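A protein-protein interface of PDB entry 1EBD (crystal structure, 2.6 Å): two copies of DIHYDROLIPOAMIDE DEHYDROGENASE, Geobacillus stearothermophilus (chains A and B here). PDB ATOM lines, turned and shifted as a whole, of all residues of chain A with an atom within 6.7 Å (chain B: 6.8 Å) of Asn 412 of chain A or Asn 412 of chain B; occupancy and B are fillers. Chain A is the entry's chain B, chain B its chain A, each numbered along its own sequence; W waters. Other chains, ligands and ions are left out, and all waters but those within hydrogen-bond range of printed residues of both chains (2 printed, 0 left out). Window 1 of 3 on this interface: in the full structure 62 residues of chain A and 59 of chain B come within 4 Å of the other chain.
OD1 of Asn 412 of chain B lies within hydrogen-bond range of ND2 of Asn 412 of chain A.
ND2 of Asn 412 of chain B lies within hydrogen-bond range of OD2 of Asp 415 of chain A (2.9 Å).
OD2 of Asp 415 of chain B sits at hydrogen-bond distance from ND2 of Asn 412 of chain A.
N of Leu 443 of chain A sits at hydrogen-bond distance from OD1 of Asp 415 of chain B (3.1 Å).
The backbone NH (N) of Leu 443 of chain B is in hydrogen-bond range of the side-chain carboxylate (OD1) of Asp 415 of chain A (3.1 Å).
Phe 376 of chain A touches none of the printed residues of chain B.
Of the printed residues of chain B, Asn 412 of chain A touches Asn 412 and Asp 415.
Of the printed residues of chain B, Asp 415 of chain A touches Asn 412 (2.9 Å) and Leu 443 (3.1 Å).
Of the printed residues of chain B, Leu 443 of chain A touches Asp 415 (3.1 Å).
Asn 412 of chain B touches just these residues of chain A: Asn 412 and Asp 415.
Of the printed residues of chain A, Asp 415 of chain B touches Asn 412 and Leu 443.
Of the printed residues of chain A, Leu 443 of chain B touches Asp 415.
The nearest residue of chain B that does not touch Asn 412 of chain A is Arg 381 of chain B (6.4 Å).
The nearest residue of chain A that does not touch Asn 412 of chain B is Ser 414 of chain A (6.3 Å).
The nearest printed residue of chain A that does not touch Asp 415 of chain B is Met 416 of chain A (4.4 Å).
Hydrophobic or aromatic side chains of chain A that line the printed part of chain B: Leu 443.
Hydrophobic or aromatic side chains of chain B within 4 Å of the printed part of chain A: Leu 443.
Among the printed residues, 5 pairs touch across the chains.
Among the printed residues, no Asp or Glu carboxylate lies within 4 Å of a Lys or Arg side-chain nitrogen of the other chain.
Asn 412 of chain B touches its own counterpart, Asn 412 of chain A.
Asn 412 of chain A touches Asp 415 of chain B, and with the chains exchanged Asp 415 of chain A touches Asn 412 of chain B.
Asp 415 of chain A touches Leu 443 of chain B, and with the chains exchanged Leu 443 of chain A touches Asp 415 of chain B.
Water W2 lies within hydrogen-bond range of the side-chain hydroxyl (OG) of Ser 414 of chain A (2.8 Å), the side-chain carboxylate (OD2) of Asp 415 of chain A (2.8 Å) and the guanidinium group (NE) of Arg 381 of chain B (3.0 Å).
Water W1 lies within hydrogen-bond range of the backbone carbonyl oxygen (O) of Asp 415 of chain B (3.2 Å) and the backbone carbonyl oxygen (O) of Asp 415 of chain A (3.2 Å).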
ATOM      1  N   GLU A 351      10.355  15.664   0.683  1.00  0.00           N
ATOM      2  CA  GLU A 351      10.500  17.076   0.381  1.00  0.00           C
ATOM      3  C   GLU A 351       9.159  17.746   0.528  1.00  0.00           C
ATOM      4  O   GLU A 351       8.118  17.099   0.395  1.00  0.00           O
ATOM      5  CB  GLU A 351      11.094  17.307  -1.015  1.00  0.00           C
ATOM      6  CG  GLU A 351      10.386  16.622  -2.171  1.00  0.00           C
ATOM      7  CD  GLU A 351      11.054  16.909  -3.511  1.00  0.00           C
ATOM      8  OE1 GLU A 351      12.066  16.266  -3.846  1.00  0.00           O
ATOM      9  OE2 GLU A 351      10.560  17.780  -4.237  1.00  0.00           O
ATOM     10  N   PHE A 376      -0.965  10.696  -0.418  1.00  0.00           N
ATOM     11  CA  PHE A 376      -0.189  10.030  -1.456  1.00  0.00           C
ATOM     12  C   PHE A 376      -0.396   8.520  -1.310  1.00  0.00           C
ATOM     13  O   PHE A 376      -0.181   7.765  -2.251  1.00  0.00           O
ATOM     14  CB  PHE A 376       1.308  10.333  -1.305  1.00  0.00           C
ATOM     15  CG  PHE A 376       1.744  11.653  -1.900  1.00  0.00           C
ATOM     16  CD1 PHE A 376       1.131  12.844  -1.537  1.00  0.00           C
ATOM     17  CD2 PHE A 376       2.807  11.706  -2.796  1.00  0.00           C
ATOM     18  CE1 PHE A 376       1.577  14.062  -2.053  1.00  0.00           C
ATOM     19  CE2 PHE A 376       3.256  12.924  -3.317  1.00  0.00           C
ATOM     20  CZ  PHE A 376       2.641  14.099  -2.942  1.00  0.00           C
ATOM     21  N   ARG A 381       1.157   6.032  -8.383  1.00  0.00           N
ATOM     22  CA  ARG A 381       2.577   6.273  -8.626  1.00  0.00           C
ATOM     23  C   ARG A 381       3.363   6.313  -7.317  1.00  0.00           C
ATOM     24  O   ARG A 381       4.486   5.821  -7.250  1.00  0.00           O
ATOM     25  CB  ARG A 381       2.750   7.583  -9.388  1.00  0.00           C
ATOM     26  CG  ARG A 381       4.179   8.064  -9.529  1.00  0.00           C
ATOM     27  CD  ARG A 381       4.655   7.937 -10.954  1.00  0.00           C
ATOM     28  NE  ARG A 381       5.271   6.641 -11.208  1.00  0.00           N
ATOM     29  CZ  ARG A 381       6.555   6.378 -10.985  1.00  0.00           C
ATOM     30  NH1 ARG A 381       7.348   7.328 -10.500  1.00  0.00           N
ATOM     31  NH2 ARG A 381       7.049   5.177 -11.264  1.00  0.00           N
ATOM     32  N   LEU A 385       6.575   4.202  -6.236  1.00  0.00           N
ATOM     33  CA  LEU A 385       7.787   4.830  -5.720  1.00  0.00           C
ATOM     34  C   LEU A 385       8.080   4.269  -4.338  1.00  0.00           C
ATOM     35  O   LEU A 385       9.202   4.358  -3.836  1.00  0.00           O
ATOM     36  CB  LEU A 385       7.574   6.340  -5.591  1.00  0.00           C
ATOM     37  CG  LEU A 385       7.268   7.149  -6.853  1.00  0.00           C
ATOM     38  CD1 LEU A 385       6.601   8.456  -6.474  1.00  0.00           C
ATOM     39  CD2 LEU A 385       8.542   7.397  -7.636  1.00  0.00           C
ATOM     40  N   ILE A 408       2.276  20.742  -0.134  1.00  0.00           N
ATOM     41  CA  ILE A 408       2.491  19.374  -0.540  1.00  0.00           C
ATOM     42  C   ILE A 408       3.675  18.862   0.218  1.00  0.00           C
ATOM     43  O   ILE A 408       4.692  19.543   0.310  1.00  0.00           O
ATOM     44  CB  ILE A 408       2.868  19.257  -2.011  1.00  0.00           C
ATOM     45  CG1 ILE A 408       2.068  20.243  -2.860  1.00  0.00           C
ATOM     46  CG2 ILE A 408       2.612  17.838  -2.465  1.00  0.00           C
ATOM     47  CD1 ILE A 408       2.541  20.341  -4.297  1.00  0.00           C
ATOM     48  N   GLY A 410       5.753  15.245   0.249  1.00  0.00           N
ATOM     49  CA  GLY A 410       5.894  13.947  -0.390  1.00  0.00           C
ATOM     50  C   GLY A 410       6.856  14.041  -1.565  1.00  0.00           C
ATOM     51  O   GLY A 410       7.330  15.139  -1.889  1.00  0.00           O
ATOM     52  N   PRO A 411       7.144  12.921  -2.251  1.00  0.00           N
ATOM     53  CA  PRO A 411       8.069  12.932  -3.392  1.00  0.00           C
ATOM     54  C   PRO A 411       7.702  13.906  -4.510  1.00  0.00           C
ATOM     55  O   PRO A 411       6.547  14.013  -4.909  1.00  0.00           O
ATOM     56  CB  PRO A 411       8.050  11.473  -3.866  1.00  0.00           C
ATOM     57  CG  PRO A 411       6.697  10.984  -3.438  1.00  0.00           C
ATOM     58  CD  PRO A 411       6.564  11.581  -2.061  1.00  0.00           C
ATOM     59  N   ASN A 412       8.696  14.656  -4.968  1.00  0.00           N
ATOM     60  CA  ASN A 412       8.523  15.613  -6.049  1.00  0.00           C
ATOM     61  C   ASN A 412       7.610  16.786  -5.743  1.00  0.00           C
ATOM     62  O   ASN A 412       7.126  17.456  -6.660  1.00  0.00           O
ATOM     63  CB  ASN A 412       8.051  14.904  -7.317  1.00  0.00           C
ATOM     64  CG  ASN A 412       9.037  13.867  -7.798  1.00  0.00           C
ATOM     65  OD1 ASN A 412      10.235  13.970  -7.535  1.00  0.00           O
ATOM     66  ND2 ASN A 412       8.541  12.844  -8.479  1.00  0.00           N
ATOM     67  N   ALA A 413       7.416  17.066  -4.460  1.00  0.00           N
ATOM     68  CA  ALA A 413       6.580  18.182  -4.042  1.00  0.00           C
ATOM     69  C   ALA A 413       7.098  19.497  -4.641  1.00  0.00           C
ATOM     70  O   ALA A 413       6.315  20.369  -5.022  1.00  0.00           O
ATOM     71  CB  ALA A 413       6.544  18.265  -2.541  1.00  0.00           C
ATOM     72  N   SER A 414       8.414  19.612  -4.787  1.00  0.00           N
ATOM     73  CA  SER A 414       9.024  20.811  -5.345  1.00  0.00           C
ATOM     74  C   SER A 414       8.639  21.060  -6.804  1.00  0.00           C
ATOM     75  O   SER A 414       8.679  22.200  -7.287  1.00  0.00           O
ATOM     76  CB  SER A 414      10.532  20.699  -5.254  1.00  0.00           C
ATOM     77  OG  SER A 414      10.970  19.573  -5.993  1.00  0.00           O
ATOM     78  N   ASP A 415       8.334  19.985  -7.524  1.00  0.00           N
ATOM     79  CA  ASP A 415       7.949  20.095  -8.929  1.00  0.00           C
ATOM     80  C   ASP A 415       6.429  20.161  -9.084  1.00  0.00           C
ATOM     81  O   ASP A 415       5.914  20.886  -9.947  1.00  0.00           O
ATOM     82  CB  ASP A 415       8.563  18.955  -9.755  1.00  0.00           C
ATOM     83  CG  ASP A 415      10.096  19.010  -9.782  1.00  0.00           C
ATOM     84  OD1 ASP A 415      10.668  20.119  -9.880  1.00  0.00           O
ATOM     85  OD2 ASP A 415      10.735  17.942  -9.697  1.00  0.00           O
ATOM     86  N   MET A 416       5.712  19.453  -8.216  1.00  0.00           N
ATOM     87  CA  MET A 416       4.252  19.465  -8.244  1.00  0.00           C
ATOM     88  C   MET A 416       3.709  20.819  -7.780  1.00  0.00           C
ATOM     89  O   MET A 416       2.577  21.193  -8.104  1.00  0.00           O
ATOM     90  CB  MET A 416       3.690  18.385  -7.328  1.00  0.00           C
ATOM     91  CG  MET A 416       4.049  16.981  -7.708  1.00  0.00           C
ATOM     92  SD  MET A 416       3.553  15.885  -6.387  1.00  0.00           S
ATOM     93  CE  MET A 416       1.820  16.210  -6.354  1.00  0.00           C
ATOM     94  N   ILE A 417       4.509  21.549  -7.010  1.00  0.00           N
ATOM     95  CA  ILE A 417       4.077  22.838  -6.497  1.00  0.00           C
ATOM     96  C   ILE A 417       3.757  23.821  -7.621  1.00  0.00           C
ATOM     97  O   ILE A 417       2.739  24.508  -7.570  1.00  0.00           O
ATOM     98  CB  ILE A 417       5.102  23.426  -5.469  1.00  0.00           C
ATOM     99  CG1 ILE A 417       4.419  24.457  -4.572  1.00  0.00           C
ATOM    100  CG2 ILE A 417       6.300  24.063  -6.169  1.00  0.00           C
ATOM    101  CD1 ILE A 417       3.186  23.932  -3.868  1.00  0.00           C
ATOM    102  N   LEU A 443       2.135  11.742  -9.869  1.00  0.00           N
ATOM    103  CA  LEU A 443       1.899  12.344  -8.564  1.00  0.00           C
ATOM    104  C   LEU A 443       1.162  13.671  -8.765  1.00  0.00           C
ATOM    105  O   LEU A 443       0.246  14.001  -8.013  1.00  0.00           O
ATOM    106  CB  LEU A 443       3.219  12.569  -7.828  1.00  0.00           C
ATOM    107  CG  LEU A 443       3.957  11.308  -7.372  1.00  0.00           C
ATOM    108  CD1 LEU A 443       5.323  11.701  -6.871  1.00  0.00           C
ATOM    109  CD2 LEU A 443       3.182  10.585  -6.288  1.00  0.00           C
ATOM    110  N   GLU B 351      12.240  10.531 -18.842  1.00  0.00           N
ATOM    111  CA  GLU B 351      10.784  10.504 -18.878  1.00  0.00           C
ATOM    112  C   GLU B 351      10.253  11.400 -20.001  1.00  0.00           C
ATOM    113  O   GLU B 351      10.835  12.448 -20.298  1.00  0.00           O
ATOM    114  CB  GLU B 351      10.250  11.015 -17.544  1.00  0.00           C
ATOM    115  CG  GLU B 351       9.304  10.098 -16.828  1.00  0.00           C
ATOM    116  CD  GLU B 351       9.004  10.594 -15.427  1.00  0.00           C
ATOM    117  OE1 GLU B 351       9.774  10.286 -14.492  1.00  0.00           O
ATOM    118  OE2 GLU B 351       8.006  11.312 -15.263  1.00  0.00           O
ATOM    119  N   PHE B 376      17.356  21.232 -20.088  1.00  0.00           N
ATOM    120  CA  PHE B 376      17.483  20.941 -18.672  1.00  0.00           C
ATOM    121  C   PHE B 376      18.924  21.239 -18.261  1.00  0.00           C
ATOM    122  O   PHE B 376      19.185  21.600 -17.123  1.00  0.00           O
ATOM    123  CB  PHE B 376      17.152  19.471 -18.387  1.00  0.00           C
ATOM    124  CG  PHE B 376      15.688  19.199 -18.223  1.00  0.00           C
ATOM    125  CD1 PHE B 376      14.800  19.428 -19.258  1.00  0.00           C
ATOM    126  CD2 PHE B 376      15.191  18.751 -17.011  1.00  0.00           C
ATOM    127  CE1 PHE B 376      13.434  19.222 -19.092  1.00  0.00           C
ATOM    128  CE2 PHE B 376      13.825  18.541 -16.836  1.00  0.00           C
ATOM    129  CZ  PHE B 376      12.947  18.781 -17.881  1.00  0.00           C
ATOM    130  N   ARG B 381      18.861  22.604 -10.869  1.00  0.00           N
ATOM    131  CA  ARG B 381      18.237  21.421 -10.291  1.00  0.00           C
ATOM    132  C   ARG B 381      18.617  20.178 -11.090  1.00  0.00           C
ATOM    133  O   ARG B 381      18.960  19.141 -10.512  1.00  0.00           O
ATOM    134  CB  ARG B 381      16.720  21.588 -10.258  1.00  0.00           C
ATOM    135  CG  ARG B 381      15.974  20.420  -9.663  1.00  0.00           C
ATOM    136  CD  ARG B 381      16.270  20.278  -8.208  1.00  0.00           C
ATOM    137  NE  ARG B 381      15.701  19.038  -7.712  1.00  0.00           N
ATOM    138  CZ  ARG B 381      16.261  18.293  -6.768  1.00  0.00           C
ATOM    139  NH1 ARG B 381      17.405  18.672  -6.204  1.00  0.00           N
ATOM    140  NH2 ARG B 381      15.704  17.142  -6.424  1.00  0.00           N
ATOM    141  N   LEU B 385      20.765  16.854  -9.992  1.00  0.00           N
ATOM    142  CA  LEU B 385      20.292  15.479 -10.149  1.00  0.00           C
ATOM    143  C   LEU B 385      21.248  14.702 -11.036  1.00  0.00           C
ATOM    144  O   LEU B 385      21.147  13.482 -11.158  1.00  0.00           O
ATOM    145  CB  LEU B 385      18.921  15.473 -10.816  1.00  0.00           C
ATOM    146  CG  LEU B 385      17.718  15.845  -9.970  1.00  0.00           C
ATOM    147  CD1 LEU B 385      16.517  16.087 -10.859  1.00  0.00           C
ATOM    148  CD2 LEU B 385      17.445  14.726  -9.016  1.00  0.00           C
ATOM    149  N   ILE B 408       7.771  17.635 -22.833  1.00  0.00           N
ATOM    150  CA  ILE B 408       8.893  17.602 -21.918  1.00  0.00           C
ATOM    151  C   ILE B 408       9.548  16.244 -21.973  1.00  0.00           C
ATOM    152  O   ILE B 408       8.868  15.221 -22.049  1.00  0.00           O
ATOM    153  CB  ILE B 408       8.452  17.786 -20.458  1.00  0.00           C
ATOM    154  CG1 ILE B 408       7.463  18.938 -20.325  1.00  0.00           C
ATOM    155  CG2 ILE B 408       9.663  18.051 -19.587  1.00  0.00           C
ATOM    156  CD1 ILE B 408       6.832  19.011 -18.966  1.00  0.00           C
ATOM    157  N   GLY B 410      12.673  14.574 -19.810  1.00  0.00           N
ATOM    158  CA  GLY B 410      13.668  14.740 -18.770  1.00  0.00           C
ATOM    159  C   GLY B 410      13.112  14.231 -17.456  1.00  0.00           C
ATOM    160  O   GLY B 410      12.033  13.632 -17.422  1.00  0.00           O
ATOM    161  N   PRO B 411      13.814  14.469 -16.344  1.00  0.00           N
ATOM    162  CA  PRO B 411      13.346  14.011 -15.036  1.00  0.00           C
ATOM    163  C   PRO B 411      12.016  14.633 -14.640  1.00  0.00           C
ATOM    164  O   PRO B 411      11.783  15.814 -14.861  1.00  0.00           O
ATOM    165  CB  PRO B 411      14.456  14.476 -14.099  1.00  0.00           C
ATOM    166  CG  PRO B 411      15.656  14.528 -14.975  1.00  0.00           C
ATOM    167  CD  PRO B 411      15.119  15.138 -16.232  1.00  0.00           C
ATOM    168  N   ASN B 412      11.141  13.817 -14.077  1.00  0.00           N
ATOM    169  CA  ASN B 412       9.847  14.266 -13.604  1.00  0.00           C
ATOM    170  C   ASN B 412       8.964  14.937 -14.615  1.00  0.00           C
ATOM    171  O   ASN B 412       8.065  15.694 -14.238  1.00  0.00           O
ATOM    172  CB  ASN B 412      10.013  15.190 -12.407  1.00  0.00           C
ATOM    173  CG  ASN B 412      10.695  14.514 -11.262  1.00  0.00           C
ATOM    174  OD1 ASN B 412      10.550  13.306 -11.069  1.00  0.00           O
ATOM    175  ND2 ASN B 412      11.476  15.270 -10.508  1.00  0.00           N
ATOM    176  N   ALA B 413       9.174  14.646 -15.891  1.00  0.00           N
ATOM    177  CA  ALA B 413       8.337  15.255 -16.913  1.00  0.00           C
ATOM    178  C   ALA B 413       6.866  14.896 -16.683  1.00  0.00           C
ATOM    179  O   ALA B 413       5.981  15.692 -16.990  1.00  0.00           O
ATOM    180  CB  ALA B 413       8.787  14.835 -18.290  1.00  0.00           C
ATOM    181  N   SER B 414       6.603  13.737 -16.079  1.00  0.00           N
ATOM    182  CA  SER B 414       5.224  13.331 -15.831  1.00  0.00           C
ATOM    183  C   SER B 414       4.565  14.194 -14.767  1.00  0.00           C
ATOM    184  O   SER B 414       3.338  14.248 -14.676  1.00  0.00           O
ATOM    185  CB  SER B 414       5.132  11.849 -15.458  1.00  0.00           C
ATOM    186  OG  SER B 414       5.750  11.575 -14.218  1.00  0.00           O
ATOM    187  N   ASP B 415       5.383  14.841 -13.942  1.00  0.00           N
ATOM    188  CA  ASP B 415       4.873  15.726 -12.898  1.00  0.00           C
ATOM    189  C   ASP B 415       4.883  17.176 -13.403  1.00  0.00           C
ATOM    190  O   ASP B 415       3.913  17.911 -13.217  1.00  0.00           O
ATOM    191  CB  ASP B 415       5.687  15.582 -11.604  1.00  0.00           C
ATOM    192  CG  ASP B 415       5.382  14.281 -10.848  1.00  0.00           C
ATOM    193  OD1 ASP B 415       4.215  13.824 -10.857  1.00  0.00           O
ATOM    194  OD2 ASP B 415       6.312  13.713 -10.230  1.00  0.00           O
ATOM    195  N   MET B 416       5.951  17.554 -14.101  1.00  0.00           N
ATOM    196  CA  MET B 416       6.080  18.900 -14.647  1.00  0.00           C
ATOM    197  C   MET B 416       4.954  19.225 -15.613  1.00  0.00           C
ATOM    198  O   MET B 416       4.458  20.348 -15.651  1.00  0.00           O
ATOM    199  CB  MET B 416       7.400  19.057 -15.402  1.00  0.00           C
ATOM    200  CG  MET B 416       8.660  18.953 -14.565  1.00  0.00           C
ATOM    201  SD  MET B 416      10.099  19.273 -15.606  1.00  0.00           S
ATOM    202  CE  MET B 416       9.674  20.877 -16.261  1.00  0.00           C
ATOM    203  N   ILE B 417       4.562  18.238 -16.405  1.00  0.00           N
ATOM    204  CA  ILE B 417       3.521  18.413 -17.410  1.00  0.00           C
ATOM    205  C   ILE B 417       2.197  18.933 -16.835  1.00  0.00           C
ATOM    206  O   ILE B 417       1.464  19.663 -17.505  1.00  0.00           O
ATOM    207  CB  ILE B 417       3.300  17.090 -18.224  1.00  0.00           C
ATOM    208  CG1 ILE B 417       2.615  17.385 -19.558  1.00  0.00           C
ATOM    209  CG2 ILE B 417       2.492  16.076 -17.421  1.00  0.00           C
ATOM    210  CD1 ILE B 417       3.447  18.259 -20.463  1.00  0.00           C
ATOM    211  N   LEU B 443      13.031  21.747 -11.146  1.00  0.00           N
ATOM    212  CA  LEU B 443      12.895  21.449 -12.564  1.00  0.00           C
ATOM    213  C   LEU B 443      11.758  22.298 -13.136  1.00  0.00           C
ATOM    214  O   LEU B 443      11.820  22.722 -14.283  1.00  0.00           O
ATOM    215  CB  LEU B 443      12.622  19.963 -12.793  1.00  0.00           C
ATOM    216  CG  LEU B 443      13.716  18.995 -12.347  1.00  0.00           C
ATOM    217  CD1 LEU B 443      13.207  17.576 -12.445  1.00  0.00           C
ATOM    218  CD2 LEU B 443      14.967  19.188 -13.182  1.00  0.00           C
HETATM  219  O   HOH W   1       3.562  20.871 -12.171  1.00  0.00           O
HETATM  220  O   HOH W   2      12.817  18.411  -7.813  1.00  0.00           O
